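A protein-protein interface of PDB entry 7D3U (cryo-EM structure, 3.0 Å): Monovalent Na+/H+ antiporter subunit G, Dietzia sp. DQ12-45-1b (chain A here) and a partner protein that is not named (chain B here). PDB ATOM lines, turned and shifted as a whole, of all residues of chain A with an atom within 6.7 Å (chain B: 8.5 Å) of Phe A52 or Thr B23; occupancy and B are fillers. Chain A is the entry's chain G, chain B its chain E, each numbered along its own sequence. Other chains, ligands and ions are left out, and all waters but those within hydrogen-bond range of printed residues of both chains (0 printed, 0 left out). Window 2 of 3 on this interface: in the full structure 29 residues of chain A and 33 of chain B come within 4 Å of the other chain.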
ATOM      1  N   GLY A  11      14.320  10.692   3.098  1.00  0.00           N
ATOM      2  CA  GLY A  11      14.039  10.103   4.392  1.00  0.00           C
ATOM      3  C   GLY A  11      15.178   9.243   4.897  1.00  0.00           C
ATOM      4  O   GLY A  11      15.459   9.214   6.096  1.00  0.00           O
ATOM      5  N   VAL A  13      18.537   9.565   4.203  1.00  0.00           N
ATOM      6  CA  VAL A  13      19.621  10.413   4.686  1.00  0.00           C
ATOM      7  C   VAL A  13      19.181  11.176   5.928  1.00  0.00           C
ATOM      8  O   VAL A  13      19.999  11.467   6.805  1.00  0.00           O
ATOM      9  CB  VAL A  13      20.116  11.361   3.570  1.00  0.00           C
ATOM     10  CG1 VAL A  13      19.016  12.298   3.122  1.00  0.00           C
ATOM     11  CG2 VAL A  13      21.347  12.133   4.023  1.00  0.00           C
ATOM     12  N   SER A  14      17.880  11.450   6.061  1.00  0.00           N
ATOM     13  CA  SER A  14      17.399  12.186   7.222  1.00  0.00           C
ATOM     14  C   SER A  14      17.427  11.327   8.479  1.00  0.00           C
ATOM     15  O   SER A  14      17.845  11.797   9.541  1.00  0.00           O
ATOM     16  CB  SER A  14      15.992  12.714   6.957  1.00  0.00           C
ATOM     17  OG  SER A  14      15.359  13.082   8.167  1.00  0.00           O
ATOM     18  N   VAL A  15      16.990  10.069   8.387  1.00  0.00           N
ATOM     19  CA  VAL A  15      17.078   9.205   9.560  1.00  0.00           C
ATOM     20  C   VAL A  15      18.533   8.916   9.898  1.00  0.00           C
ATOM     21  O   VAL A  15      18.882   8.778  11.075  1.00  0.00           O
ATOM     22  CB  VAL A  15      16.271   7.905   9.378  1.00  0.00           C
ATOM     23  CG1 VAL A  15      14.839   8.213   9.006  1.00  0.00           C
ATOM     24  CG2 VAL A  15      16.907   7.000   8.346  1.00  0.00           C
ATOM     25  N   LEU A  16      19.415   8.859   8.896  1.00  0.00           N
ATOM     26  CA  LEU A  16      20.827   8.673   9.212  1.00  0.00           C
ATOM     27  C   LEU A  16      21.393   9.889   9.939  1.00  0.00           C
ATOM     28  O   LEU A  16      22.124   9.744  10.927  1.00  0.00           O
ATOM     29  CB  LEU A  16      21.619   8.384   7.940  1.00  0.00           C
ATOM     30  CG  LEU A  16      21.847   6.900   7.660  1.00  0.00           C
ATOM     31  CD1 LEU A  16      22.890   6.721   6.574  1.00  0.00           C
ATOM     32  CD2 LEU A  16      22.258   6.170   8.927  1.00  0.00           C
ATOM     33  N   VAL A  17      21.054  11.093   9.472  1.00  0.00           N
ATOM     34  CA  VAL A  17      21.506  12.311  10.138  1.00  0.00           C
ATOM     35  C   VAL A  17      20.959  12.378  11.557  1.00  0.00           C
ATOM     36  O   VAL A  17      21.676  12.733  12.497  1.00  0.00           O
ATOM     37  CB  VAL A  17      21.102  13.546   9.311  1.00  0.00           C
ATOM     38  CG1 VAL A  17      21.155  14.804  10.159  1.00  0.00           C
ATOM     39  CG2 VAL A  17      22.005  13.680   8.097  1.00  0.00           C
ATOM     40  N   GLY A  18      19.685  12.027  11.736  1.00  0.00           N
ATOM     41  CA  GLY A  18      19.098  12.059  13.065  1.00  0.00           C
ATOM     42  C   GLY A  18      19.733  11.060  14.013  1.00  0.00           C
ATOM     43  O   GLY A  18      19.965  11.367  15.186  1.00  0.00           O
ATOM     44  N   ALA A  19      20.026   9.854  13.525  1.00  0.00           N
ATOM     45  CA  ALA A  19      20.698   8.873  14.369  1.00  0.00           C
ATOM     46  C   ALA A  19      22.102   9.334  14.732  1.00  0.00           C
ATOM     47  O   ALA A  19      22.547   9.156  15.871  1.00  0.00           O
ATOM     48  CB  ALA A  19      20.742   7.518  13.667  1.00  0.00           C
ATOM     49  N   VAL A  21      23.060  12.414  15.013  1.00  0.00           N
ATOM     50  CA  VAL A  21      22.908  13.494  15.983  1.00  0.00           C
ATOM     51  C   VAL A  21      22.586  12.938  17.361  1.00  0.00           C
ATOM     52  O   VAL A  21      23.082  13.436  18.376  1.00  0.00           O
ATOM     53  CB  VAL A  21      21.835  14.485  15.508  1.00  0.00           C
ATOM     54  CG1 VAL A  21      21.465  15.445  16.621  1.00  0.00           C
ATOM     55  CG2 VAL A  21      22.338  15.238  14.310  1.00  0.00           C
ATOM     56  N   GLY A  47      16.391  17.430  20.289  1.00  0.00           N
ATOM     57  CA  GLY A  47      15.402  18.049  19.434  1.00  0.00           C
ATOM     58  C   GLY A  47      15.683  17.820  17.965  1.00  0.00           C
ATOM     59  O   GLY A  47      14.837  17.277  17.245  1.00  0.00           O
ATOM     60  N   LEU A  48      16.872  18.227  17.509  1.00  0.00           N
ATOM     61  CA  LEU A  48      17.205  18.111  16.094  1.00  0.00           C
ATOM     62  C   LEU A  48      17.204  16.661  15.635  1.00  0.00           C
ATOM     63  O   LEU A  48      16.585  16.325  14.619  1.00  0.00           O
ATOM     64  CB  LEU A  48      18.558  18.763  15.811  1.00  0.00           C
ATOM     65  CG  LEU A  48      18.639  20.275  16.024  1.00  0.00           C
ATOM     66  CD1 LEU A  48      20.072  20.745  15.846  1.00  0.00           C
ATOM     67  CD2 LEU A  48      17.711  21.040  15.094  1.00  0.00           C
ATOM     68  N   GLY A  49      17.925  15.790  16.346  1.00  0.00           N
ATOM     69  CA  GLY A  49      17.990  14.399  15.932  1.00  0.00           C
ATOM     70  C   GLY A  49      16.624  13.748  15.855  1.00  0.00           C
ATOM     71  O   GLY A  49      16.324  13.024  14.904  1.00  0.00           O
ATOM     72  N   LEU A  50      15.765  14.020  16.838  1.00  0.00           N
ATOM     73  CA  LEU A  50      14.453  13.386  16.845  1.00  0.00           C
ATOM     74  C   LEU A  50      13.555  13.946  15.748  1.00  0.00           C
ATOM     75  O   LEU A  50      12.804  13.194  15.120  1.00  0.00           O
ATOM     76  CB  LEU A  50      13.794  13.538  18.213  1.00  0.00           C
ATOM     77  CG  LEU A  50      12.455  12.814  18.343  1.00  0.00           C
ATOM     78  CD1 LEU A  50      12.541  11.420  17.771  1.00  0.00           C
ATOM     79  CD2 LEU A  50      11.996  12.752  19.780  1.00  0.00           C
ATOM     80  N   VAL A  51      13.616  15.254  15.494  1.00  0.00           N
ATOM     81  CA  VAL A  51      12.831  15.811  14.396  1.00  0.00           C
ATOM     82  C   VAL A  51      13.294  15.227  13.068  1.00  0.00           C
ATOM     83  O   VAL A  51      12.478  14.898  12.194  1.00  0.00           O
ATOM     84  CB  VAL A  51      12.913  17.348  14.404  1.00  0.00           C
ATOM     85  CG1 VAL A  51      12.425  17.916  13.082  1.00  0.00           C
ATOM     86  CG2 VAL A  51      12.101  17.905  15.556  1.00  0.00           C
ATOM     87  N   PHE A  52      14.609  15.063  12.907  1.00  0.00           N
ATOM     88  CA  PHE A  52      15.143  14.467  11.687  1.00  0.00           C
ATOM     89  C   PHE A  52      14.656  13.034  11.523  1.00  0.00           C
ATOM     90  O   PHE A  52      14.238  12.631  10.432  1.00  0.00           O
ATOM     91  CB  PHE A  52      16.669  14.515  11.706  1.00  0.00           C
ATOM     92  CG  PHE A  52      17.241  15.752  11.087  1.00  0.00           C
ATOM     93  CD1 PHE A  52      17.209  15.935   9.719  1.00  0.00           C
ATOM     94  CD2 PHE A  52      17.810  16.733  11.874  1.00  0.00           C
ATOM     95  CE1 PHE A  52      17.733  17.074   9.150  1.00  0.00           C
ATOM     96  CE2 PHE A  52      18.334  17.871  11.311  1.00  0.00           C
ATOM     97  CZ  PHE A  52      18.296  18.043   9.948  1.00  0.00           C
ATOM     98  N   VAL A  53      14.708  12.248  12.600  1.00  0.00           N
ATOM     99  CA  VAL A  53      14.262  10.859  12.525  1.00  0.00           C
ATOM    100  C   VAL A  53      12.775  10.788  12.209  1.00  0.00           C
ATOM    101  O   VAL A  53      12.338   9.957  11.406  1.00  0.00           O
ATOM    102  CB  VAL A  53      14.604  10.113  13.825  1.00  0.00           C
ATOM    103  CG1 VAL A  53      14.053   8.709  13.782  1.00  0.00           C
ATOM    104  CG2 VAL A  53      16.103  10.059  14.018  1.00  0.00           C
ATOM    105  N   ILE A  54      11.974  11.666  12.818  1.00  0.00           N
ATOM    106  CA  ILE A  54      10.535  11.655  12.570  1.00  0.00           C
ATOM    107  C   ILE A  54      10.245  11.972  11.109  1.00  0.00           C
ATOM    108  O   ILE A  54       9.473  11.270  10.444  1.00  0.00           O
ATOM    109  CB  ILE A  54       9.820  12.639  13.512  1.00  0.00           C
ATOM    110  CG1 ILE A  54       9.809  12.095  14.937  1.00  0.00           C
ATOM    111  CG2 ILE A  54       8.403  12.898  13.039  1.00  0.00           C
ATOM    112  CD1 ILE A  54       9.309  10.688  15.044  1.00  0.00           C
ATOM    113  N   ALA A  55      10.867  13.030  10.585  1.00  0.00           N
ATOM    114  CA  ALA A  55      10.599  13.417   9.203  1.00  0.00           C
ATOM    115  C   ALA A  55      11.101  12.364   8.223  1.00  0.00           C
ATOM    116  O   ALA A  55      10.441  12.083   7.217  1.00  0.00           O
ATOM    117  CB  ALA A  55      11.229  14.773   8.905  1.00  0.00           C
ATOM    118  N   GLY A  56      12.257  11.760   8.501  1.00  0.00           N
ATOM    119  CA  GLY A  56      12.756  10.718   7.620  1.00  0.00           C
ATOM    120  C   GLY A  56      11.880   9.482   7.632  1.00  0.00           C
ATOM    121  O   GLY A  56      11.607   8.891   6.583  1.00  0.00           O
ATOM    122  N   ALA A  57      11.427   9.072   8.818  1.00  0.00           N
ATOM    123  CA  ALA A  57      10.483   7.968   8.911  1.00  0.00           C
ATOM    124  C   ALA A  57       9.212   8.272   8.131  1.00  0.00           C
ATOM    125  O   ALA A  57       8.683   7.404   7.429  1.00  0.00           O
ATOM    126  CB  ALA A  57      10.163   7.682  10.376  1.00  0.00           C
ATOM    127  N   GLN A  77       8.110  18.497  19.491  1.00  0.00           N
ATOM    128  CA  GLN A  77       9.403  17.938  19.862  1.00  0.00           C
ATOM    129  C   GLN A  77      10.427  19.037  20.087  1.00  0.00           C
ATOM    130  O   GLN A  77      11.187  18.994  21.057  1.00  0.00           O
ATOM    131  CB  GLN A  77       9.893  16.977  18.782  1.00  0.00           C
ATOM    132  CG  GLN A  77       9.060  15.725  18.652  1.00  0.00           C
ATOM    133  CD  GLN A  77       9.532  14.833  17.526  1.00  0.00           C
ATOM    134  OE1 GLN A  77      10.149  15.293  16.571  1.00  0.00           O
ATOM    135  NE2 GLN A  77       9.243  13.547  17.630  1.00  0.00           N
ATOM    136  N   PHE A  78      10.461  20.030  19.198  1.00  0.00           N
ATOM    137  CA  PHE A  78      11.403  21.132  19.367  1.00  0.00           C
ATOM    138  C   PHE A  78      11.150  21.869  20.676  1.00  0.00           C
ATOM    139  O   PHE A  78      12.061  22.035  21.503  1.00  0.00           O
ATOM    140  CB  PHE A  78      11.309  22.089  18.180  1.00  0.00           C
ATOM    141  CG  PHE A  78      12.186  21.709  17.028  1.00  0.00           C
ATOM    142  CD1 PHE A  78      13.511  21.374  17.234  1.00  0.00           C
ATOM    143  CD2 PHE A  78      11.688  21.680  15.738  1.00  0.00           C
ATOM    144  CE1 PHE A  78      14.322  21.021  16.178  1.00  0.00           C
ATOM    145  CE2 PHE A  78      12.496  21.329  14.678  1.00  0.00           C
ATOM    146  CZ  PHE A  78      13.815  20.998  14.899  1.00  0.00           C
ATOM    147  N   LEU B  15      10.158  23.877   3.973  1.00  0.00           N
ATOM    148  CA  LEU B  15      10.617  22.848   4.902  1.00  0.00           C
ATOM    149  C   LEU B  15      11.963  22.277   4.483  1.00  0.00           C
ATOM    150  O   LEU B  15      12.763  21.890   5.339  1.00  0.00           O
ATOM    151  CB  LEU B  15       9.584  21.729   5.039  1.00  0.00           C
ATOM    152  CG  LEU B  15       8.164  22.111   5.458  1.00  0.00           C
ATOM    153  CD1 LEU B  15       7.143  21.186   4.815  1.00  0.00           C
ATOM    154  CD2 LEU B  15       8.016  22.112   6.973  1.00  0.00           C
ATOM    155  N   LEU B  16      12.253  22.229   3.183  1.00  0.00           N
ATOM    156  CA  LEU B  16      13.560  21.722   2.778  1.00  0.00           C
ATOM    157  C   LEU B  16      14.661  22.721   3.121  1.00  0.00           C
ATOM    158  O   LEU B  16      15.738  22.333   3.592  1.00  0.00           O
ATOM    159  CB  LEU B  16      13.561  21.389   1.291  1.00  0.00           C
ATOM    160  CG  LEU B  16      14.809  20.670   0.776  1.00  0.00           C
ATOM    161  CD1 LEU B  16      14.438  19.716  -0.350  1.00  0.00           C
ATOM    162  CD2 LEU B  16      15.867  21.667   0.324  1.00  0.00           C
ATOM    163  N   TRP B  17      14.407  24.014   2.907  1.00  0.00           N
ATOM    164  CA  TRP B  17      15.351  25.029   3.361  1.00  0.00           C
ATOM    165  C   TRP B  17      15.526  24.973   4.873  1.00  0.00           C
ATOM    166  O   TRP B  17      16.642  25.125   5.387  1.00  0.00           O
ATOM    167  CB  TRP B  17      14.881  26.420   2.927  1.00  0.00           C
ATOM    168  CG  TRP B  17      15.580  27.526   3.647  1.00  0.00           C
ATOM    169  CD1 TRP B  17      16.728  28.156   3.262  1.00  0.00           C
ATOM    170  CD2 TRP B  17      15.181  28.137   4.879  1.00  0.00           C
ATOM    171  NE1 TRP B  17      17.066  29.122   4.178  1.00  0.00           N
ATOM    172  CE2 TRP B  17      16.133  29.129   5.181  1.00  0.00           C
ATOM    173  CE3 TRP B  17      14.111  27.939   5.757  1.00  0.00           C
ATOM    174  CZ2 TRP B  17      16.047  29.922   6.321  1.00  0.00           C
ATOM    175  CZ3 TRP B  17      14.028  28.726   6.889  1.00  0.00           C
ATOM    176  CH2 TRP B  17      14.990  29.706   7.162  1.00  0.00           C
ATOM    177  N   PHE B  18      14.426  24.764   5.602  1.00  0.00           N
ATOM    178  CA  PHE B  18      14.500  24.634   7.051  1.00  0.00           C
ATOM    179  C   PHE B  18      15.347  23.437   7.447  1.00  0.00           C
ATOM    180  O   PHE B  18      16.133  23.510   8.395  1.00  0.00           O
ATOM    181  CB  PHE B  18      13.090  24.515   7.631  1.00  0.00           C
ATOM    182  CG  PHE B  18      13.053  24.180   9.097  1.00  0.00           C
ATOM    183  CD1 PHE B  18      13.123  25.181  10.050  1.00  0.00           C
ATOM    184  CD2 PHE B  18      12.919  22.868   9.520  1.00  0.00           C
ATOM    185  CE1 PHE B  18      13.080  24.878  11.397  1.00  0.00           C
ATOM    186  CE2 PHE B  18      12.877  22.560  10.865  1.00  0.00           C
ATOM    187  CZ  PHE B  18      12.957  23.566  11.804  1.00  0.00           C
ATOM    188  N   PHE B  19      15.222  22.331   6.717  1.00  0.00           N
ATOM    189  CA  PHE B  19      15.992  21.148   7.069  1.00  0.00           C
ATOM    190  C   PHE B  19      17.459  21.306   6.704  1.00  0.00           C
ATOM    191  O   PHE B  19      18.315  20.701   7.347  1.00  0.00           O
ATOM    192  CB  PHE B  19      15.391  19.912   6.411  1.00  0.00           C
ATOM    193  CG  PHE B  19      14.396  19.207   7.279  1.00  0.00           C
ATOM    194  CD1 PHE B  19      13.275  19.872   7.740  1.00  0.00           C
ATOM    195  CD2 PHE B  19      14.593  17.894   7.661  1.00  0.00           C
ATOM    196  CE1 PHE B  19      12.360  19.239   8.548  1.00  0.00           C
ATOM    197  CE2 PHE B  19      13.679  17.257   8.471  1.00  0.00           C
ATOM    198  CZ  PHE B  19      12.561  17.933   8.915  1.00  0.00           C
ATOM    199  N   TRP B  20      17.779  22.141   5.716  1.00  0.00           N
ATOM    200  CA  TRP B  20      19.189  22.451   5.482  1.00  0.00           C
ATOM    201  C   TRP B  20      19.747  23.330   6.600  1.00  0.00           C
ATOM    202  O   TRP B  20      20.833  23.065   7.140  1.00  0.00           O
ATOM    203  CB  TRP B  20      19.381  23.124   4.123  1.00  0.00           C
ATOM    204  CG  TRP B  20      20.770  22.936   3.593  1.00  0.00           C
ATOM    205  CD1 TRP B  20      21.237  21.876   2.875  1.00  0.00           C
ATOM    206  CD2 TRP B  20      21.881  23.823   3.768  1.00  0.00           C
ATOM    207  NE1 TRP B  20      22.567  22.052   2.579  1.00  0.00           N
ATOM    208  CE2 TRP B  20      22.987  23.240   3.116  1.00  0.00           C
ATOM    209  CE3 TRP B  20      22.048  25.056   4.405  1.00  0.00           C
ATOM    210  CZ2 TRP B  20      24.240  23.848   3.084  1.00  0.00           C
ATOM    211  CZ3 TRP B  20      23.293  25.658   4.371  1.00  0.00           C
ATOM    212  CH2 TRP B  20      24.372  25.054   3.716  1.00  0.00           C
ATOM    213  N   GLN B  21      19.010  24.384   6.963  1.00  0.00           N
ATOM    214  CA  GLN B  21      19.432  25.241   8.064  1.00  0.00           C
ATOM    215  C   GLN B  21      19.427  24.506   9.396  1.00  0.00           C
ATOM    216  O   GLN B  21      19.991  25.011  10.373  1.00  0.00           O
ATOM    217  CB  GLN B  21      18.534  26.475   8.149  1.00  0.00           C
ATOM    218  N   GLN B  22      18.790  23.338   9.462  1.00  0.00           N
ATOM    219  CA  GLN B  22      18.843  22.517  10.662  1.00  0.00           C
ATOM    220  C   GLN B  22      19.916  21.441  10.600  1.00  0.00           C
ATOM    221  O   GLN B  22      20.458  21.072  11.642  1.00  0.00           O
ATOM    222  CB  GLN B  22      17.487  21.856  10.927  1.00  0.00           C
ATOM    223  CG  GLN B  22      16.400  22.815  11.387  1.00  0.00           C
ATOM    224  CD  GLN B  22      16.939  23.969  12.206  1.00  0.00           C
ATOM    225  OE1 GLN B  22      17.071  25.087  11.710  1.00  0.00           O
ATOM    226  NE2 GLN B  22      17.248  23.705  13.470  1.00  0.00           N
ATOM    227  N   THR B  23      20.248  20.915   9.416  1.00  0.00           N
ATOM    228  CA  THR B  23      21.348  19.960   9.362  1.00  0.00           C
ATOM    229  C   THR B  23      22.684  20.663   9.532  1.00  0.00           C
ATOM    230  O   THR B  23      23.643  20.050  10.012  1.00  0.00           O
ATOM    231  CB  THR B  23      21.343  19.152   8.062  1.00  0.00           C
ATOM    232  OG1 THR B  23      22.528  18.350   8.004  1.00  0.00           O
ATOM    233  CG2 THR B  23      21.343  20.055   6.860  1.00  0.00           C
ATOM    234  N   THR B  24      22.773  21.947   9.177  1.00  0.00           N
ATOM    235  CA  THR B  24      23.989  22.679   9.530  1.00  0.00           C
ATOM    236  C   THR B  24      24.113  22.823  11.046  1.00  0.00           C
ATOM    237  O   THR B  24      25.203  22.649  11.608  1.00  0.00           O
ATOM    238  CB  THR B  24      24.030  24.034   8.813  1.00  0.00           C
ATOM    239  OG1 THR B  24      25.363  24.559   8.856  1.00  0.00           O
ATOM    240  CG2 THR B  24      23.061  25.044   9.418  1.00  0.00           C
ATOM    241  N   THR B  25      22.993  23.063  11.733  1.00  0.00           N
ATOM    242  CA  THR B  25      22.997  23.094  13.192  1.00  0.00           C
ATOM    243  C   THR B  25      23.307  21.719  13.776  1.00  0.00           C
ATOM    244  O   THR B  25      23.986  21.614  14.800  1.00  0.00           O
ATOM    245  CB  THR B  25      21.648  23.617  13.690  1.00  0.00           C
ATOM    246  OG1 THR B  25      21.597  25.041  13.526  1.00  0.00           O
ATOM    247  CG2 THR B  25      21.417  23.273  15.151  1.00  0.00           C
ATOM    248  N   SER B  26      22.844  20.657  13.121  1.00  0.00           N
ATOM    249  CA  SER B  26      23.114  19.305  13.594  1.00  0.00           C
ATOM    250  C   SER B  26      24.587  18.948  13.445  1.00  0.00           C
ATOM    251  O   SER B  26      25.172  18.310  14.329  1.00  0.00           O
ATOM    252  CB  SER B  26      22.241  18.317  12.830  1.00  0.00           C
ATOM    253  OG  SER B  26      20.872  18.510  13.134  1.00  0.00           O
ATOM    254  N   ALA B  27      25.200  19.332  12.324  1.00  0.00           N
ATOM    255  CA  ALA B  27      26.637  19.151  12.175  1.00  0.00           C
ATOM    256  C   ALA B  27      27.392  19.971  13.207  1.00  0.00           C
ATOM    257  O   ALA B  27      28.419  19.526  13.731  1.00  0.00           O
ATOM    258  CB  ALA B  27      27.072  19.528  10.760  1.00  0.00           C
ATOM    259  N   LYS B  28      26.888  21.166  13.527  1.00  0.00           N
ATOM    260  CA  LYS B  28      27.479  21.943  14.613  1.00  0.00           C
ATOM    261  C   LYS B  28      27.391  21.197  15.938  1.00  0.00           C
ATOM    262  O   LYS B  28      28.347  21.192  16.719  1.00  0.00           O
ATOM    263  CB  LYS B  28      26.794  23.304  14.721  1.00  0.00           C
ATOM    264  CG  LYS B  28      27.659  24.373  15.361  1.00  0.00           C
ATOM    265  CD  LYS B  28      26.955  25.718  15.404  1.00  0.00           C
ATOM    266  CE  LYS B  28      26.251  26.030  14.094  1.00  0.00           C
ATOM    267  NZ  LYS B  28      27.193  26.050  12.942  1.00  0.00           N
ATOM    268  N   VAL B  29      26.248  20.564  16.206  1.00  0.00           N
ATOM    269  CA  VAL B  29      26.081  19.796  17.440  1.00  0.00           C
ATOM    270  C   VAL B  29      27.084  18.651  17.490  1.00  0.00           C
ATOM    271  O   VAL B  29      27.766  18.437  18.500  1.00  0.00           O
ATOM    272  CB  VAL B  29      24.639  19.271  17.559  1.00  0.00           C
ATOM    273  CG1 VAL B  29      24.540  18.240  18.670  1.00  0.00           C
ATOM    274  CG2 VAL B  29      23.673  20.408  17.803  1.00  0.00           C
ATOM    275  N   VAL B  30      27.179  17.893  16.397  1.00  0.00           N
ATOM    276  CA  VAL B  30      28.083  16.746  16.352  1.00  0.00           C
ATOM    277  C   VAL B  30      29.529  17.195  16.531  1.00  0.00           C
ATOM    278  O   VAL B  30      30.304  16.563  17.258  1.00  0.00           O
ATOM    279  CB  VAL B  30      27.883  15.963  15.041  1.00  0.00           C
ATOM    280  CG1 VAL B  30      29.106  15.122  14.724  1.00  0.00           C
ATOM    281  CG2 VAL B  30      26.648  15.087  15.140  1.00  0.00           C
ATOM    282  N   ARG B  31      29.874  18.346  15.945  1.00  0.00           N
ATOM    283  CA  ARG B  31      31.240  18.904  16.141  1.00  0.00           C
ATOM    284  C   ARG B  31      31.405  19.290  17.613  1.00  0.00           C
ATOM    285  O   ARG B  31      32.501  19.062  18.154  1.00  0.00           O
ATOM    286  CB  ARG B  31      31.449  20.137  15.257  1.00  0.00           C
ATOM    287  CG  ARG B  31      31.783  19.818  13.808  1.00  0.00           C
ATOM    288  CD  ARG B  31      31.912  21.083  12.982  1.00  0.00           C
ATOM    289  NE  ARG B  31      30.778  21.314  12.099  1.00  0.00           N
ATOM    290  CZ  ARG B  31      30.098  22.452  12.035  1.00  0.00           C
ATOM    291  NH1 ARG B  31      30.430  23.467  12.814  1.00  0.00           N
ATOM    292  NH2 ARG B  31      29.082  22.571  11.198  1.00  0.00           N
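Of the 22 printed residues of chain A, 5 touch a printed residue of chain B. Hydrophobic or aromatic side chains of chain A that line the printed part of chain B: Val A21, Leu A48, Phe A52, Ala A55 and Phe A78. Printed residues of chain B that touch a printed residue of chain A: Phe B18, Phe B19, Gln B22, Thr B23, Thr B25 and Ser B26. Hydrophobic or aromatic side chains of chain B that line the printed part of chain A: Phe B18 and Phe B19. Among the printed residues, no Asp or Glu carboxylate lies within 4 Å of a Lys or Arg side-chain nitrogen of the other chain.
Ser A14 touches none of the printed residues of chain B. Printed residues of chain B within 4 Å of Val A21: Ser B26 (3.4 Å). Phe A52 touches just these residues of chain B: Phe B19, Gln B22, Thr B23 and Ser B26. Gly A56 touches none of the printed residues of chain B. Printed residues of chain A within 4 Å of Gln B22: Leu A48 (3.2 Å) and Phe A52 (3.8 Å). Of the printed residues of chain A, Thr B25 touches Leu A48 (2.9 Å). The nearest residue of chain B that does not touch Phe A52 is Trp B20 (5.9 Å). The nearest residue of chain A that does not touch Thr B23 is Val A17 (4.4 Å).
OG of Ser A14 lies within hydrogen-bond range of O of Phe A52, 2.6 Å away. The side-chain hydroxyl (OG) of Ser B26 lies within hydrogen-bond range of the backbone carbonyl oxygen (O) of Gln B22 (3.0 Å).
Ser B26 touches Val A21 (CB to CG2, 3.4 Å). NE2 of Gln B22 touches CD2 of Leu A48, at 3.2 Å. Leu A48 touches Thr B25 (CD1 to CG2, 2.9 Å). Leu A48 touches Ser B26 (CB to OG, 3.5 Å). Phe B19 touches Phe A52 (CD2 to CE1, 3.6 Å). CZ of Phe A52 touches C of Gln B22, 3.8 Å away. Thr B23 touches Phe A52. Phe A52 touches Ser B26 (CE2 to OG, 3.2 Å). Phe B19 touches Ala A55 (CZ to CB, 3.4 Å). Phe B18 touches Phe A78 (CZ to CE2, 3.7 Å).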
